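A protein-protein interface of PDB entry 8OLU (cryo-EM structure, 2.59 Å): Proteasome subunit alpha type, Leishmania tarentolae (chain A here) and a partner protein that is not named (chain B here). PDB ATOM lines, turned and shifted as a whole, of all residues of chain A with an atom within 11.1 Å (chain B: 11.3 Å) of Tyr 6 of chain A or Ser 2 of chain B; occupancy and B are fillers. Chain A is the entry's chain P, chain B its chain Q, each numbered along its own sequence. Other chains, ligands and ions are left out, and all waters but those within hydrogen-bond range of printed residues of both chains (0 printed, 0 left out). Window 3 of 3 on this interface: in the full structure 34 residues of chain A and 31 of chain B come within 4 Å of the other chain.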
ATOM      1  N   GLU A   3     -25.525   6.944  10.992  1.00  0.00           N
ATOM      2  CA  GLU A   3     -26.115   6.126  12.092  1.00  0.00           C
ATOM      3  C   GLU A   3     -25.322   4.814  12.279  1.00  0.00           C
ATOM      4  O   GLU A   3     -25.672   4.038  13.178  1.00  0.00           O
ATOM      5  CB  GLU A   3     -27.625   5.890  11.849  1.00  0.00           C
ATOM      6  CG  GLU A   3     -28.400   5.400  13.090  1.00  0.00           C
ATOM      7  CD  GLU A   3     -29.814   4.844  12.920  1.00  0.00           C
ATOM      8  OE1 GLU A   3     -30.692   5.582  12.383  1.00  0.00           O
ATOM      9  OE2 GLU A   3     -30.056   3.690  13.381  1.00  0.00           O
ATOM     10  N   ALA A   4     -24.279   4.536  11.455  1.00  0.00           N
ATOM     11  CA  ALA A   4     -23.369   3.421  11.734  1.00  0.00           C
ATOM     12  C   ALA A   4     -22.212   3.934  12.574  1.00  0.00           C
ATOM     13  O   ALA A   4     -21.616   4.946  12.250  1.00  0.00           O
ATOM     14  CB  ALA A   4     -22.846   2.759  10.502  1.00  0.00           C
ATOM     15  N   PHE A   5     -21.972   3.315  13.720  1.00  0.00           N
ATOM     16  CA  PHE A   5     -21.050   3.938  14.643  1.00  0.00           C
ATOM     17  C   PHE A   5     -19.903   3.008  14.968  1.00  0.00           C
ATOM     18  O   PHE A   5     -19.030   3.370  15.759  1.00  0.00           O
ATOM     19  CB  PHE A   5     -21.741   4.312  15.950  1.00  0.00           C
ATOM     20  CG  PHE A   5     -22.555   5.567  15.896  1.00  0.00           C
ATOM     21  CD1 PHE A   5     -21.935   6.804  15.920  1.00  0.00           C
ATOM     22  CD2 PHE A   5     -23.944   5.495  15.837  1.00  0.00           C
ATOM     23  CE1 PHE A   5     -22.701   7.965  15.852  1.00  0.00           C
ATOM     24  CE2 PHE A   5     -24.706   6.650  15.759  1.00  0.00           C
ATOM     25  CZ  PHE A   5     -24.084   7.882  15.767  1.00  0.00           C
ATOM     26  N   TYR A   6     -19.946   1.819  14.424  1.00  0.00           N
ATOM     27  CA  TYR A   6     -18.824   0.954  14.610  1.00  0.00           C
ATOM     28  C   TYR A   6     -17.718   1.338  13.661  1.00  0.00           C
ATOM     29  O   TYR A   6     -17.967   2.007  12.674  1.00  0.00           O
ATOM     30  CB  TYR A   6     -19.228  -0.470  14.356  1.00  0.00           C
ATOM     31  CG  TYR A   6     -19.803  -0.754  13.003  1.00  0.00           C
ATOM     32  CD1 TYR A   6     -18.991  -0.982  11.904  1.00  0.00           C
ATOM     33  CD2 TYR A   6     -21.162  -0.897  12.855  1.00  0.00           C
ATOM     34  CE1 TYR A   6     -19.535  -1.380  10.695  1.00  0.00           C
ATOM     35  CE2 TYR A   6     -21.722  -1.268  11.652  1.00  0.00           C
ATOM     36  CZ  TYR A   6     -20.914  -1.486  10.558  1.00  0.00           C
ATOM     37  OH  TYR A   6     -21.498  -1.818   9.365  1.00  0.00           O
ATOM     38  N   GLY A   7     -16.503   0.941  13.978  1.00  0.00           N
ATOM     39  CA  GLY A   7     -15.370   1.308  13.180  1.00  0.00           C
ATOM     40  C   GLY A   7     -15.200   0.363  12.012  1.00  0.00           C
ATOM     41  O   GLY A   7     -15.465  -0.811  12.168  1.00  0.00           O
ATOM     42  N   LEU A   8     -14.698   0.898  10.884  1.00  0.00           N
ATOM     43  CA  LEU A   8     -14.527   0.161   9.636  1.00  0.00           C
ATOM     44  C   LEU A   8     -13.067  -0.200   9.445  1.00  0.00           C
ATOM     45  O   LEU A   8     -12.741  -1.269   8.908  1.00  0.00           O
ATOM     46  CB  LEU A   8     -14.989   1.030   8.467  1.00  0.00           C
ATOM     47  CG  LEU A   8     -16.461   1.447   8.545  1.00  0.00           C
ATOM     48  CD1 LEU A   8     -16.876   2.293   7.370  1.00  0.00           C
ATOM     49  CD2 LEU A   8     -17.339   0.209   8.637  1.00  0.00           C
ATOM     50  N   THR A   9     -12.214   0.688   9.934  1.00  0.00           N
ATOM     51  CA  THR A   9     -10.794   0.451  10.008  1.00  0.00           C
ATOM     52  C   THR A   9     -10.497  -0.150  11.353  1.00  0.00           C
ATOM     53  O   THR A   9     -10.871   0.468  12.353  1.00  0.00           O
ATOM     54  CB  THR A   9      -9.978   1.731   9.892  1.00  0.00           C
ATOM     55  OG1 THR A   9     -10.320   2.413   8.678  1.00  0.00           O
ATOM     56  CG2 THR A   9      -8.487   1.500   9.934  1.00  0.00           C
ATOM     57  N   THR A  10      -9.864  -1.342  11.301  1.00  0.00           N
ATOM     58  CA  THR A  10      -9.502  -2.131  12.455  1.00  0.00           C
ATOM     59  C   THR A  10      -8.179  -2.841  12.263  1.00  0.00           C
ATOM     60  O   THR A  10      -7.733  -3.022  11.144  1.00  0.00           O
ATOM     61  CB  THR A  10     -10.500  -3.251  12.699  1.00  0.00           C
ATOM     62  OG1 THR A  10     -10.598  -4.182  11.616  1.00  0.00           O
ATOM     63  CG2 THR A  10     -11.863  -2.674  13.002  1.00  0.00           C
ATOM     64  N   GLN A  19      -7.697  -1.409   5.979  1.00  0.00           N
ATOM     65  CA  GLN A  19      -8.391  -0.358   5.269  1.00  0.00           C
ATOM     66  C   GLN A  19      -7.457   0.795   4.957  1.00  0.00           C
ATOM     67  O   GLN A  19      -7.629   1.444   3.950  1.00  0.00           O
ATOM     68  CB  GLN A  19      -9.575   0.258   6.016  1.00  0.00           C
ATOM     69  CG  GLN A  19     -10.899  -0.450   5.786  1.00  0.00           C
ATOM     70  CD  GLN A  19     -11.151  -0.719   4.324  1.00  0.00           C
ATOM     71  OE1 GLN A  19     -11.447   0.208   3.581  1.00  0.00           O
ATOM     72  NE2 GLN A  19     -11.029  -1.957   3.901  1.00  0.00           N
ATOM     73  N   GLU A 118      -8.661  10.972  12.172  1.00  0.00           N
ATOM     74  CA  GLU A 118     -10.016  10.714  12.626  1.00  0.00           C
ATOM     75  C   GLU A 118     -10.680   9.727  11.683  1.00  0.00           C
ATOM     76  O   GLU A 118     -11.363   8.852  12.162  1.00  0.00           O
ATOM     77  CB  GLU A 118     -11.071  11.802  12.577  1.00  0.00           C
ATOM     78  CG  GLU A 118     -10.818  13.060  13.368  1.00  0.00           C
ATOM     79  CD  GLU A 118     -11.731  14.214  12.887  1.00  0.00           C
ATOM     80  OE1 GLU A 118     -12.842  13.940  12.322  1.00  0.00           O
ATOM     81  OE2 GLU A 118     -11.319  15.407  13.018  1.00  0.00           O
ATOM     82  N   PHE A 119     -10.504   9.821  10.378  1.00  0.00           N
ATOM     83  CA  PHE A 119     -11.230   8.890   9.547  1.00  0.00           C
ATOM     84  C   PHE A 119     -10.597   7.501   9.553  1.00  0.00           C
ATOM     85  O   PHE A 119     -11.095   6.617   8.887  1.00  0.00           O
ATOM     86  CB  PHE A 119     -11.450   9.448   8.153  1.00  0.00           C
ATOM     87  CG  PHE A 119     -12.543  10.488   8.108  1.00  0.00           C
ATOM     88  CD1 PHE A 119     -13.760  10.222   7.509  1.00  0.00           C
ATOM     89  CD2 PHE A 119     -12.364  11.741   8.682  1.00  0.00           C
ATOM     90  CE1 PHE A 119     -14.764  11.187   7.495  1.00  0.00           C
ATOM     91  CE2 PHE A 119     -13.366  12.698   8.696  1.00  0.00           C
ATOM     92  CZ  PHE A 119     -14.564  12.423   8.084  1.00  0.00           C
ATOM     93  N   THR A 120      -9.584   7.248  10.389  1.00  0.00           N
ATOM     94  CA  THR A 120      -8.996   5.920  10.498  1.00  0.00           C
ATOM     95  C   THR A 120      -9.451   5.242  11.786  1.00  0.00           C
ATOM     96  O   THR A 120      -8.976   4.169  12.122  1.00  0.00           O
ATOM     97  CB  THR A 120      -7.460   5.995  10.548  1.00  0.00           C
ATOM     98  OG1 THR A 120      -7.001   6.638  11.740  1.00  0.00           O
ATOM     99  CG2 THR A 120      -6.875   6.761   9.391  1.00  0.00           C
ATOM    100  N   GLN A 121     -10.257   5.943  12.569  1.00  0.00           N
ATOM    101  CA  GLN A 121     -10.585   5.460  13.889  1.00  0.00           C
ATOM    102  C   GLN A 121     -12.061   5.673  14.169  1.00  0.00           C
ATOM    103  O   GLN A 121     -12.702   4.726  14.575  1.00  0.00           O
ATOM    104  CB  GLN A 121      -9.735   6.184  14.936  1.00  0.00           C
ATOM    105  CG  GLN A 121      -9.963   5.754  16.381  1.00  0.00           C
ATOM    106  CD  GLN A 121      -8.709   5.968  17.183  1.00  0.00           C
ATOM    107  OE1 GLN A 121      -8.091   7.025  17.089  1.00  0.00           O
ATOM    108  NE2 GLN A 121      -8.287   4.952  17.918  1.00  0.00           N
ATOM    109  N   SER A 122     -12.573   6.886  13.973  1.00  0.00           N
ATOM    110  CA  SER A 122     -13.987   7.193  14.116  1.00  0.00           C
ATOM    111  C   SER A 122     -14.865   6.151  13.472  1.00  0.00           C
ATOM    112  O   SER A 122     -14.489   5.535  12.483  1.00  0.00           O
ATOM    113  CB  SER A 122     -14.376   8.512  13.493  1.00  0.00           C
ATOM    114  OG  SER A 122     -14.438   9.519  14.486  1.00  0.00           O
ATOM    115  N   GLY A 123     -16.082   6.082  13.987  1.00  0.00           N
ATOM    116  CA  GLY A 123     -17.007   5.061  13.542  1.00  0.00           C
ATOM    117  C   GLY A 123     -17.749   5.466  12.289  1.00  0.00           C
ATOM    118  O   GLY A 123     -17.952   6.639  12.012  1.00  0.00           O
ATOM    119  N   GLY A 124     -18.071   4.455  11.516  1.00  0.00           N
ATOM    120  CA  GLY A 124     -18.876   4.652  10.333  1.00  0.00           C
ATOM    121  C   GLY A 124     -18.115   5.066   9.087  1.00  0.00           C
ATOM    122  O   GLY A 124     -18.627   4.977   8.005  1.00  0.00           O
ATOM    123  N   VAL A 125     -16.882   5.484   9.179  1.00  0.00           N
ATOM    124  CA  VAL A 125     -16.304   6.122   8.032  1.00  0.00           C
ATOM    125  C   VAL A 125     -15.174   5.274   7.544  1.00  0.00           C
ATOM    126  O   VAL A 125     -14.624   4.517   8.313  1.00  0.00           O
ATOM    127  CB  VAL A 125     -15.790   7.492   8.424  1.00  0.00           C
ATOM    128  CG1 VAL A 125     -16.952   8.450   8.710  1.00  0.00           C
ATOM    129  CG2 VAL A 125     -14.887   7.377   9.634  1.00  0.00           C
ATOM    130  N   ARG A 126     -14.883   5.363   6.266  1.00  0.00           N
ATOM    131  CA  ARG A 126     -13.680   4.761   5.764  1.00  0.00           C
ATOM    132  C   ARG A 126     -12.638   5.856   5.754  1.00  0.00           C
ATOM    133  O   ARG A 126     -12.980   7.011   5.722  1.00  0.00           O
ATOM    134  CB  ARG A 126     -13.890   4.263   4.333  1.00  0.00           C
ATOM    135  CG  ARG A 126     -14.230   5.368   3.360  1.00  0.00           C
ATOM    136  CD  ARG A 126     -14.001   4.907   1.971  1.00  0.00           C
ATOM    137  NE  ARG A 126     -14.647   5.843   1.040  1.00  0.00           N
ATOM    138  CZ  ARG A 126     -14.192   7.054   0.726  1.00  0.00           C
ATOM    139  NH1 ARG A 126     -14.937   7.874   0.021  1.00  0.00           N
ATOM    140  NH2 ARG A 126     -12.992   7.430   1.121  1.00  0.00           N
ATOM    141  N   PRO A 127     -11.356   5.556   5.656  1.00  0.00           N
ATOM    142  CA  PRO A 127     -10.380   6.586   5.443  1.00  0.00           C
ATOM    143  C   PRO A 127     -10.399   7.273   4.086  1.00  0.00           C
ATOM    144  O   PRO A 127     -10.966   6.790   3.112  1.00  0.00           O
ATOM    145  CB  PRO A 127      -9.070   5.797   5.423  1.00  0.00           C
ATOM    146  CG  PRO A 127      -9.388   4.591   6.206  1.00  0.00           C
ATOM    147  CD  PRO A 127     -10.775   4.231   5.737  1.00  0.00           C
ATOM    148  N   SER B   2     -26.369  -2.847   8.453  1.00  0.00           N
ATOM    149  CA  SER B   2     -25.037  -2.337   8.858  1.00  0.00           C
ATOM    150  C   SER B   2     -24.518  -3.216  10.001  1.00  0.00           C
ATOM    151  O   SER B   2     -23.328  -3.525   9.974  1.00  0.00           O
ATOM    152  CB  SER B   2     -24.973  -0.803   9.182  1.00  0.00           C
ATOM    153  OG  SER B   2     -23.874  -0.157   8.505  1.00  0.00           O
ATOM    154  N   HIS B   3     -25.342  -3.695  10.953  1.00  0.00           N
ATOM    155  CA  HIS B   3     -24.795  -4.509  12.055  1.00  0.00           C
ATOM    156  C   HIS B   3     -24.120  -5.815  11.585  1.00  0.00           C
ATOM    157  O   HIS B   3     -23.393  -6.407  12.352  1.00  0.00           O
ATOM    158  CB  HIS B   3     -25.842  -4.826  13.146  1.00  0.00           C
ATOM    159  CG  HIS B   3     -26.719  -6.016  12.850  1.00  0.00           C
ATOM    160  ND1 HIS B   3     -27.823  -5.974  12.015  1.00  0.00           N
ATOM    161  CD2 HIS B   3     -26.592  -7.314  13.282  1.00  0.00           C
ATOM    162  CE1 HIS B   3     -28.347  -7.199  11.924  1.00  0.00           C
ATOM    163  NE2 HIS B   3     -27.600  -8.047  12.711  1.00  0.00           N
ATOM    164  N   ARG B   4     -24.351  -6.301  10.357  1.00  0.00           N
ATOM    165  CA  ARG B   4     -23.746  -7.545   9.892  1.00  0.00           C
ATOM    166  C   ARG B   4     -22.250  -7.343   9.671  1.00  0.00           C
ATOM    167  O   ARG B   4     -21.497  -8.302   9.573  1.00  0.00           O
ATOM    168  CB  ARG B   4     -24.336  -8.017   8.553  1.00  0.00           C
ATOM    169  CG  ARG B   4     -25.864  -8.067   8.498  1.00  0.00           C
ATOM    170  CD  ARG B   4     -26.488  -8.255   7.105  1.00  0.00           C
ATOM    171  NE  ARG B   4     -26.506  -9.649   6.637  1.00  0.00           N
ATOM    172  CZ  ARG B   4     -25.598 -10.207   5.827  1.00  0.00           C
ATOM    173  NH1 ARG B   4     -25.549 -11.521   5.696  1.00  0.00           N
ATOM    174  NH2 ARG B   4     -24.708  -9.460   5.188  1.00  0.00           N
ATOM    175  N   TYR B   5     -21.855  -6.077   9.548  1.00  0.00           N
ATOM    176  CA  TYR B   5     -20.524  -5.681   9.130  1.00  0.00           C
ATOM    177  C   TYR B   5     -19.753  -5.116  10.329  1.00  0.00           C
ATOM    178  O   TYR B   5     -18.692  -4.517  10.183  1.00  0.00           O
ATOM    179  CB  TYR B   5     -20.590  -4.681   7.949  1.00  0.00           C
ATOM    180  CG  TYR B   5     -21.466  -5.101   6.782  1.00  0.00           C
ATOM    181  CD1 TYR B   5     -21.303  -6.332   6.148  1.00  0.00           C
ATOM    182  CD2 TYR B   5     -22.525  -4.307   6.356  1.00  0.00           C
ATOM    183  CE1 TYR B   5     -22.158  -6.748   5.133  1.00  0.00           C
ATOM    184  CE2 TYR B   5     -23.388  -4.707   5.344  1.00  0.00           C
ATOM    185  CZ  TYR B   5     -23.219  -5.941   4.744  1.00  0.00           C
ATOM    186  OH  TYR B   5     -24.090  -6.316   3.746  1.00  0.00           O
ATOM    187  N   ASP B   6     -20.284  -5.263  11.541  1.00  0.00           N
ATOM    188  CA  ASP B   6     -19.604  -4.730  12.711  1.00  0.00           C
ATOM    189  C   ASP B   6     -18.598  -5.798  13.097  1.00  0.00           C
ATOM    190  O   ASP B   6     -18.963  -6.975  13.221  1.00  0.00           O
ATOM    191  CB  ASP B   6     -20.618  -4.377  13.803  1.00  0.00           C
ATOM    192  CG  ASP B   6     -20.063  -3.798  15.104  1.00  0.00           C
ATOM    193  OD1 ASP B   6     -18.857  -3.714  15.223  1.00  0.00           O
ATOM    194  OD2 ASP B   6     -20.871  -3.467  16.024  1.00  0.00           O
ATOM    195  N   SER B   7     -17.349  -5.362  13.277  1.00  0.00           N
ATOM    196  CA  SER B   7     -16.242  -6.243  13.622  1.00  0.00           C
ATOM    197  C   SER B   7     -16.053  -6.398  15.139  1.00  0.00           C
ATOM    198  O   SER B   7     -15.196  -7.174  15.563  1.00  0.00           O
ATOM    199  CB  SER B   7     -15.007  -5.694  13.016  1.00  0.00           C
ATOM    200  OG  SER B   7     -14.816  -4.337  13.462  1.00  0.00           O
ATOM    201  N   ARG B   8     -16.824  -5.655  15.951  1.00  0.00           N
ATOM    202  CA  ARG B   8     -17.023  -5.955  17.360  1.00  0.00           C
ATOM    203  C   ARG B   8     -15.673  -5.832  18.094  1.00  0.00           C
ATOM    204  O   ARG B   8     -15.140  -6.734  18.740  1.00  0.00           O
ATOM    205  CB  ARG B   8     -17.764  -7.301  17.407  1.00  0.00           C
ATOM    206  CG  ARG B   8     -19.284  -7.197  17.538  1.00  0.00           C
ATOM    207  CD  ARG B   8     -20.049  -8.326  16.862  1.00  0.00           C
ATOM    208  NE  ARG B   8     -19.320  -9.595  16.847  1.00  0.00           N
ATOM    209  CZ  ARG B   8     -18.987 -10.288  15.758  1.00  0.00           C
ATOM    210  NH1 ARG B   8     -19.248  -9.812  14.552  1.00  0.00           N
ATOM    211  NH2 ARG B   8     -18.381 -11.460  15.888  1.00  0.00           N
ATOM    212  N   THR B   9     -15.079  -4.664  17.939  1.00  0.00           N
ATOM    213  CA  THR B   9     -13.748  -4.396  18.411  1.00  0.00           C
ATOM    214  C   THR B   9     -13.640  -4.472  19.935  1.00  0.00           C
ATOM    215  O   THR B   9     -12.639  -4.921  20.469  1.00  0.00           O
ATOM    216  CB  THR B   9     -13.384  -2.978  18.000  1.00  0.00           C
ATOM    217  OG1 THR B   9     -14.363  -2.038  18.452  1.00  0.00           O
ATOM    218  CG2 THR B   9     -13.229  -2.879  16.508  1.00  0.00           C
ATOM    219  N   THR B  10     -14.653  -3.989  20.642  1.00  0.00           N
ATOM    220  CA  THR B  10     -14.629  -4.062  22.088  1.00  0.00           C
ATOM    221  C   THR B  10     -15.309  -5.338  22.602  1.00  0.00           C
ATOM    222  O   THR B  10     -16.040  -5.270  23.563  1.00  0.00           O
ATOM    223  CB  THR B  10     -15.291  -2.815  22.693  1.00  0.00           C
ATOM    224  OG1 THR B  10     -16.700  -2.682  22.462  1.00  0.00           O
ATOM    225  CG2 THR B  10     -14.666  -1.545  22.166  1.00  0.00           C
ATOM    226  N   THR B  11     -15.174  -6.486  21.962  1.00  0.00           N
ATOM    227  CA  THR B  11     -15.746  -7.660  22.580  1.00  0.00           C
ATOM    228  C   THR B  11     -14.620  -8.471  23.132  1.00  0.00           C
ATOM    229  O   THR B  11     -13.502  -8.279  22.682  1.00  0.00           O
ATOM    230  CB  THR B  11     -16.474  -8.637  21.647  1.00  0.00           C
ATOM    231  OG1 THR B  11     -15.701  -9.021  20.503  1.00  0.00           O
ATOM    232  CG2 THR B  11     -17.787  -8.041  21.200  1.00  0.00           C
ATOM    233  N   GLN B  20      -8.441  -6.952  19.275  1.00  0.00           N
ATOM    234  CA  GLN B  20      -7.963  -5.707  18.736  1.00  0.00           C
ATOM    235  C   GLN B  20      -6.794  -5.165  19.532  1.00  0.00           C
ATOM    236  O   GLN B  20      -5.929  -4.522  18.936  1.00  0.00           O
ATOM    237  CB  GLN B  20      -8.995  -4.578  18.712  1.00  0.00           C
ATOM    238  CG  GLN B  20      -9.920  -4.566  17.489  1.00  0.00           C
ATOM    239  CD  GLN B  20      -9.311  -5.026  16.195  1.00  0.00           C
ATOM    240  OE1 GLN B  20      -8.789  -4.213  15.461  1.00  0.00           O
ATOM    241  NE2 GLN B  20      -9.416  -6.324  15.928  1.00  0.00           N
ATOM    242  N   TYR B 127     -11.118   2.994  24.696  1.00  0.00           N
ATOM    243  CA  TYR B 127     -11.336   2.501  23.365  1.00  0.00           C
ATOM    244  C   TYR B 127     -11.293   0.986  23.324  1.00  0.00           C
ATOM    245  O   TYR B 127     -11.561   0.397  22.295  1.00  0.00           O
ATOM    246  CB  TYR B 127     -10.309   3.168  22.449  1.00  0.00           C
ATOM    247  CG  TYR B 127     -10.709   4.560  22.028  1.00  0.00           C
ATOM    248  CD1 TYR B 127     -10.912   4.864  20.696  1.00  0.00           C
ATOM    249  CD2 TYR B 127     -10.927   5.573  22.934  1.00  0.00           C
ATOM    250  CE1 TYR B 127     -11.274   6.133  20.263  1.00  0.00           C
ATOM    251  CE2 TYR B 127     -11.291   6.853  22.529  1.00  0.00           C
ATOM    252  CZ  TYR B 127     -11.476   7.135  21.185  1.00  0.00           C
ATOM    253  OH  TYR B 127     -11.835   8.366  20.701  1.00  0.00           O
ATOM    254  N   TYR B 130     -15.595   0.793  25.413  1.00  0.00           N
ATOM    255  CA  TYR B 130     -16.739   1.513  24.872  1.00  0.00           C
ATOM    256  C   TYR B 130     -16.411   1.809  23.427  1.00  0.00           C
ATOM    257  O   TYR B 130     -15.257   1.949  23.075  1.00  0.00           O
ATOM    258  CB  TYR B 130     -17.003   2.836  25.641  1.00  0.00           C
ATOM    259  CG  TYR B 130     -17.258   2.593  27.107  1.00  0.00           C
ATOM    260  CD1 TYR B 130     -16.234   2.587  28.033  1.00  0.00           C
ATOM    261  CD2 TYR B 130     -18.515   2.221  27.568  1.00  0.00           C
ATOM    262  CE1 TYR B 130     -16.454   2.253  29.371  1.00  0.00           C
ATOM    263  CE2 TYR B 130     -18.763   1.907  28.905  1.00  0.00           C
ATOM    264  CZ  TYR B 130     -17.723   1.911  29.816  1.00  0.00           C
ATOM    265  OH  TYR B 130     -17.964   1.588  31.137  1.00  0.00           O
ATOM    266  N   GLY B 131     -17.430   1.936  22.586  1.00  0.00           N
ATOM    267  CA  GLY B 131     -17.344   2.851  21.450  1.00  0.00           C
ATOM    268  C   GLY B 131     -17.274   2.123  20.120  1.00  0.00           C
ATOM    269  O   GLY B 131     -17.437   2.736  19.066  1.00  0.00           O
ATOM    270  N   GLY B 132     -17.054   0.814  20.176  1.00  0.00           N
ATOM    271  CA  GLY B 132     -17.049   0.054  18.932  1.00  0.00           C
ATOM    272  C   GLY B 132     -16.028   0.460  17.859  1.00  0.00           C
ATOM    273  O   GLY B 132     -16.042  -0.164  16.819  1.00  0.00           O
ATOM    274  N   VAL B 133     -15.061   1.322  18.140  1.00  0.00           N
ATOM    275  CA  VAL B 133     -13.974   1.572  17.210  1.00  0.00           C
ATOM    276  C   VAL B 133     -12.690   0.856  17.598  1.00  0.00           C
ATOM    277  O   VAL B 133     -12.714   0.023  18.472  1.00  0.00           O
ATOM    278  CB  VAL B 133     -13.764   3.086  17.048  1.00  0.00           C
ATOM    279  CG1 VAL B 133     -15.036   3.733  16.505  1.00  0.00           C
ATOM    280  CG2 VAL B 133     -13.309   3.833  18.292  1.00  0.00           C
ATOM    281  N   ARG B 134     -11.592   1.020  16.865  1.00  0.00           N
ATOM    282  CA  ARG B 134     -10.378   0.224  17.132  1.00  0.00           C
ATOM    283  C   ARG B 134      -9.604   0.953  18.198  1.00  0.00           C
ATOM    284  O   ARG B 134      -9.884   2.110  18.411  1.00  0.00           O
ATOM    285  CB  ARG B 134      -9.428   0.076  15.942  1.00  0.00           C
ATOM    286  CG  ARG B 134      -8.910   1.407  15.458  1.00  0.00           C
ATOM    287  CD  ARG B 134      -7.953   1.316  14.303  1.00  0.00           C
ATOM    288  NE  ARG B 134      -7.558   2.676  13.950  1.00  0.00           N
ATOM    289  CZ  ARG B 134      -6.465   3.294  14.403  1.00  0.00           C
ATOM    290  NH1 ARG B 134      -5.717   2.796  15.380  1.00  0.00           N
ATOM    291  NH2 ARG B 134      -6.189   4.481  13.903  1.00  0.00           N
ATOM    292  N   PRO B 135      -8.689   0.324  18.935  1.00  0.00           N
ATOM    293  CA  PRO B 135      -7.867   1.035  19.880  1.00  0.00           C
ATOM    294  C   PRO B 135      -6.783   1.894  19.256  1.00  0.00           C
ATOM    295  O   PRO B 135      -6.508   1.813  18.063  1.00  0.00           O
ATOM    296  CB  PRO B 135      -7.212  -0.064  20.701  1.00  0.00           C
ATOM    297  CG  PRO B 135      -7.305  -1.253  19.906  1.00  0.00           C
ATOM    298  CD  PRO B 135      -8.516  -1.111  19.052  1.00  0.00           C
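The side-chain hydroxyl (OH) of Tyr 6 of chain A is in hydrogen-bond range of the backbone carbonyl oxygen (O) of Ser 2 of chain B (2.6 Å). The backbone carbonyl oxygen of Gly 132 of chain B is in hydrogen-bond range of the backbone NH of Gly 7 of chain A (3.1 Å). The guanidinium group (NE) of Arg 134 of chain B lies within hydrogen-bond range of the backbone carbonyl oxygen (O) of Thr 120 of chain A (2.8 Å). O of Arg 134 of chain B sits at hydrogen-bond distance from NE2 of Gln 121 of chain A, at 3.3 Å.
N of Gly 124 of chain A sits at hydrogen-bond distance from O of Tyr 6 of chain A (2.7 Å). The backbone NH (N) of Arg 8 of chain B lies within hydrogen-bond range of the side-chain carboxylate (OD1) of Asp 6 of chain B (2.9 Å). OG1 of Thr 9 of chain B lies within hydrogen-bond range of O of Gly 132 of chain B (3.0 Å). The backbone carbonyl oxygen (O) of Val 133 of chain B is in hydrogen-bond range of the side-chain hydroxyl (OG1) of Thr 9 of chain B (2.6 Å).
Tyr 5 of chain B touches Tyr 6 of chain A. Tyr 6 of chain A touches Asp 6 of chain B (CB to OD1, 3.4 Å). OG of Ser 7 of chain B touches O of Gly 7 of chain A, 3.8 Å away. O of Thr 9 of chain A touches CD of Arg 134 of chain B (3.6 Å). Ser 7 of chain B touches Thr 10 of chain A (OG to CG2, 3.4 Å). Thr 9 of chain B touches Thr 10 of chain A (CG2 to CG2, 3.8 Å). Gln 20 of chain B touches Thr 10 of chain A. Gln 121 of chain A touches Tyr 127 of chain B. O of Pro 135 of chain B touches NE2 of Gln 121 of chain A, at 3.6 Å. Gly 123 of chain A touches Val 133 of chain B (N to CG1, 3.6 Å).
Ala 4 of chain A touches just one residue of chain B: Ser 2 (3.7 Å). Tyr 6 of chain A touches just these residues of chain B: Ser 2 (2.6 Å), Tyr 5 (3.3 Å), Asp 6 (3.4 Å) and Gly 132 (3.7 Å). Leu 8 of chain A touches none of the printed residues of chain B. Of the printed residues of chain B, Thr 9 of chain A touches Arg 134 (3.6 Å). Phe 119 of chain A touches none of the printed residues of chain B. Of the printed residues of chain B, Gln 121 of chain A touches Tyr 127 (3.8 Å), Val 133 (3.2 Å), Arg 134 (3.3 Å) and Pro 135 (3.6 Å). Of chain B, only Val 133 (3.6 Å) comes within 4 Å of Gly 123 of chain A. No residue of chain B comes within 4 Å of Gly 124 of chain A. Ser 2 of chain B touches two residues of chain A. Tyr 5 of chain B touches just one residue of chain A: Tyr 6. Of chain A, only Tyr 6 (3.4 Å) comes within 4 Å of Asp 6 of chain B. Arg 8 of chain B touches none of the printed residues of chain A. Printed residues of chain A within 4 Å of Tyr 127 of chain B: Gln 121. Of the printed residues of chain A, Pro 135 of chain B touches Gln 121. The nearest printed residue of chain A that does not touch Gln 20 of chain B is Thr 9 of chain A (6.0 Å).
Printed residues of chain B that touch a printed residue of chain A: Ser 2, Tyr 5, Asp 6, Ser 7, Thr 9, Gln 20, Tyr 127, Gly 131, Gly 132, Val 133, Arg 134 and Pro 135. Hydrophobic or aromatic side chains of chain B that line the printed part of chain A: Tyr 5, Tyr 127 and Val 133. Hydrophobic or aromatic side chains of chain A within 4 Å of the printed part of chain B: Ala 4 and Tyr 6. Among the printed residues, 19 pairs touch across the chains. Among the printed residues, no Asp or Glu carboxylate lies within 4 Å of a Lys or Arg side-chain nitrogen of the other chain.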
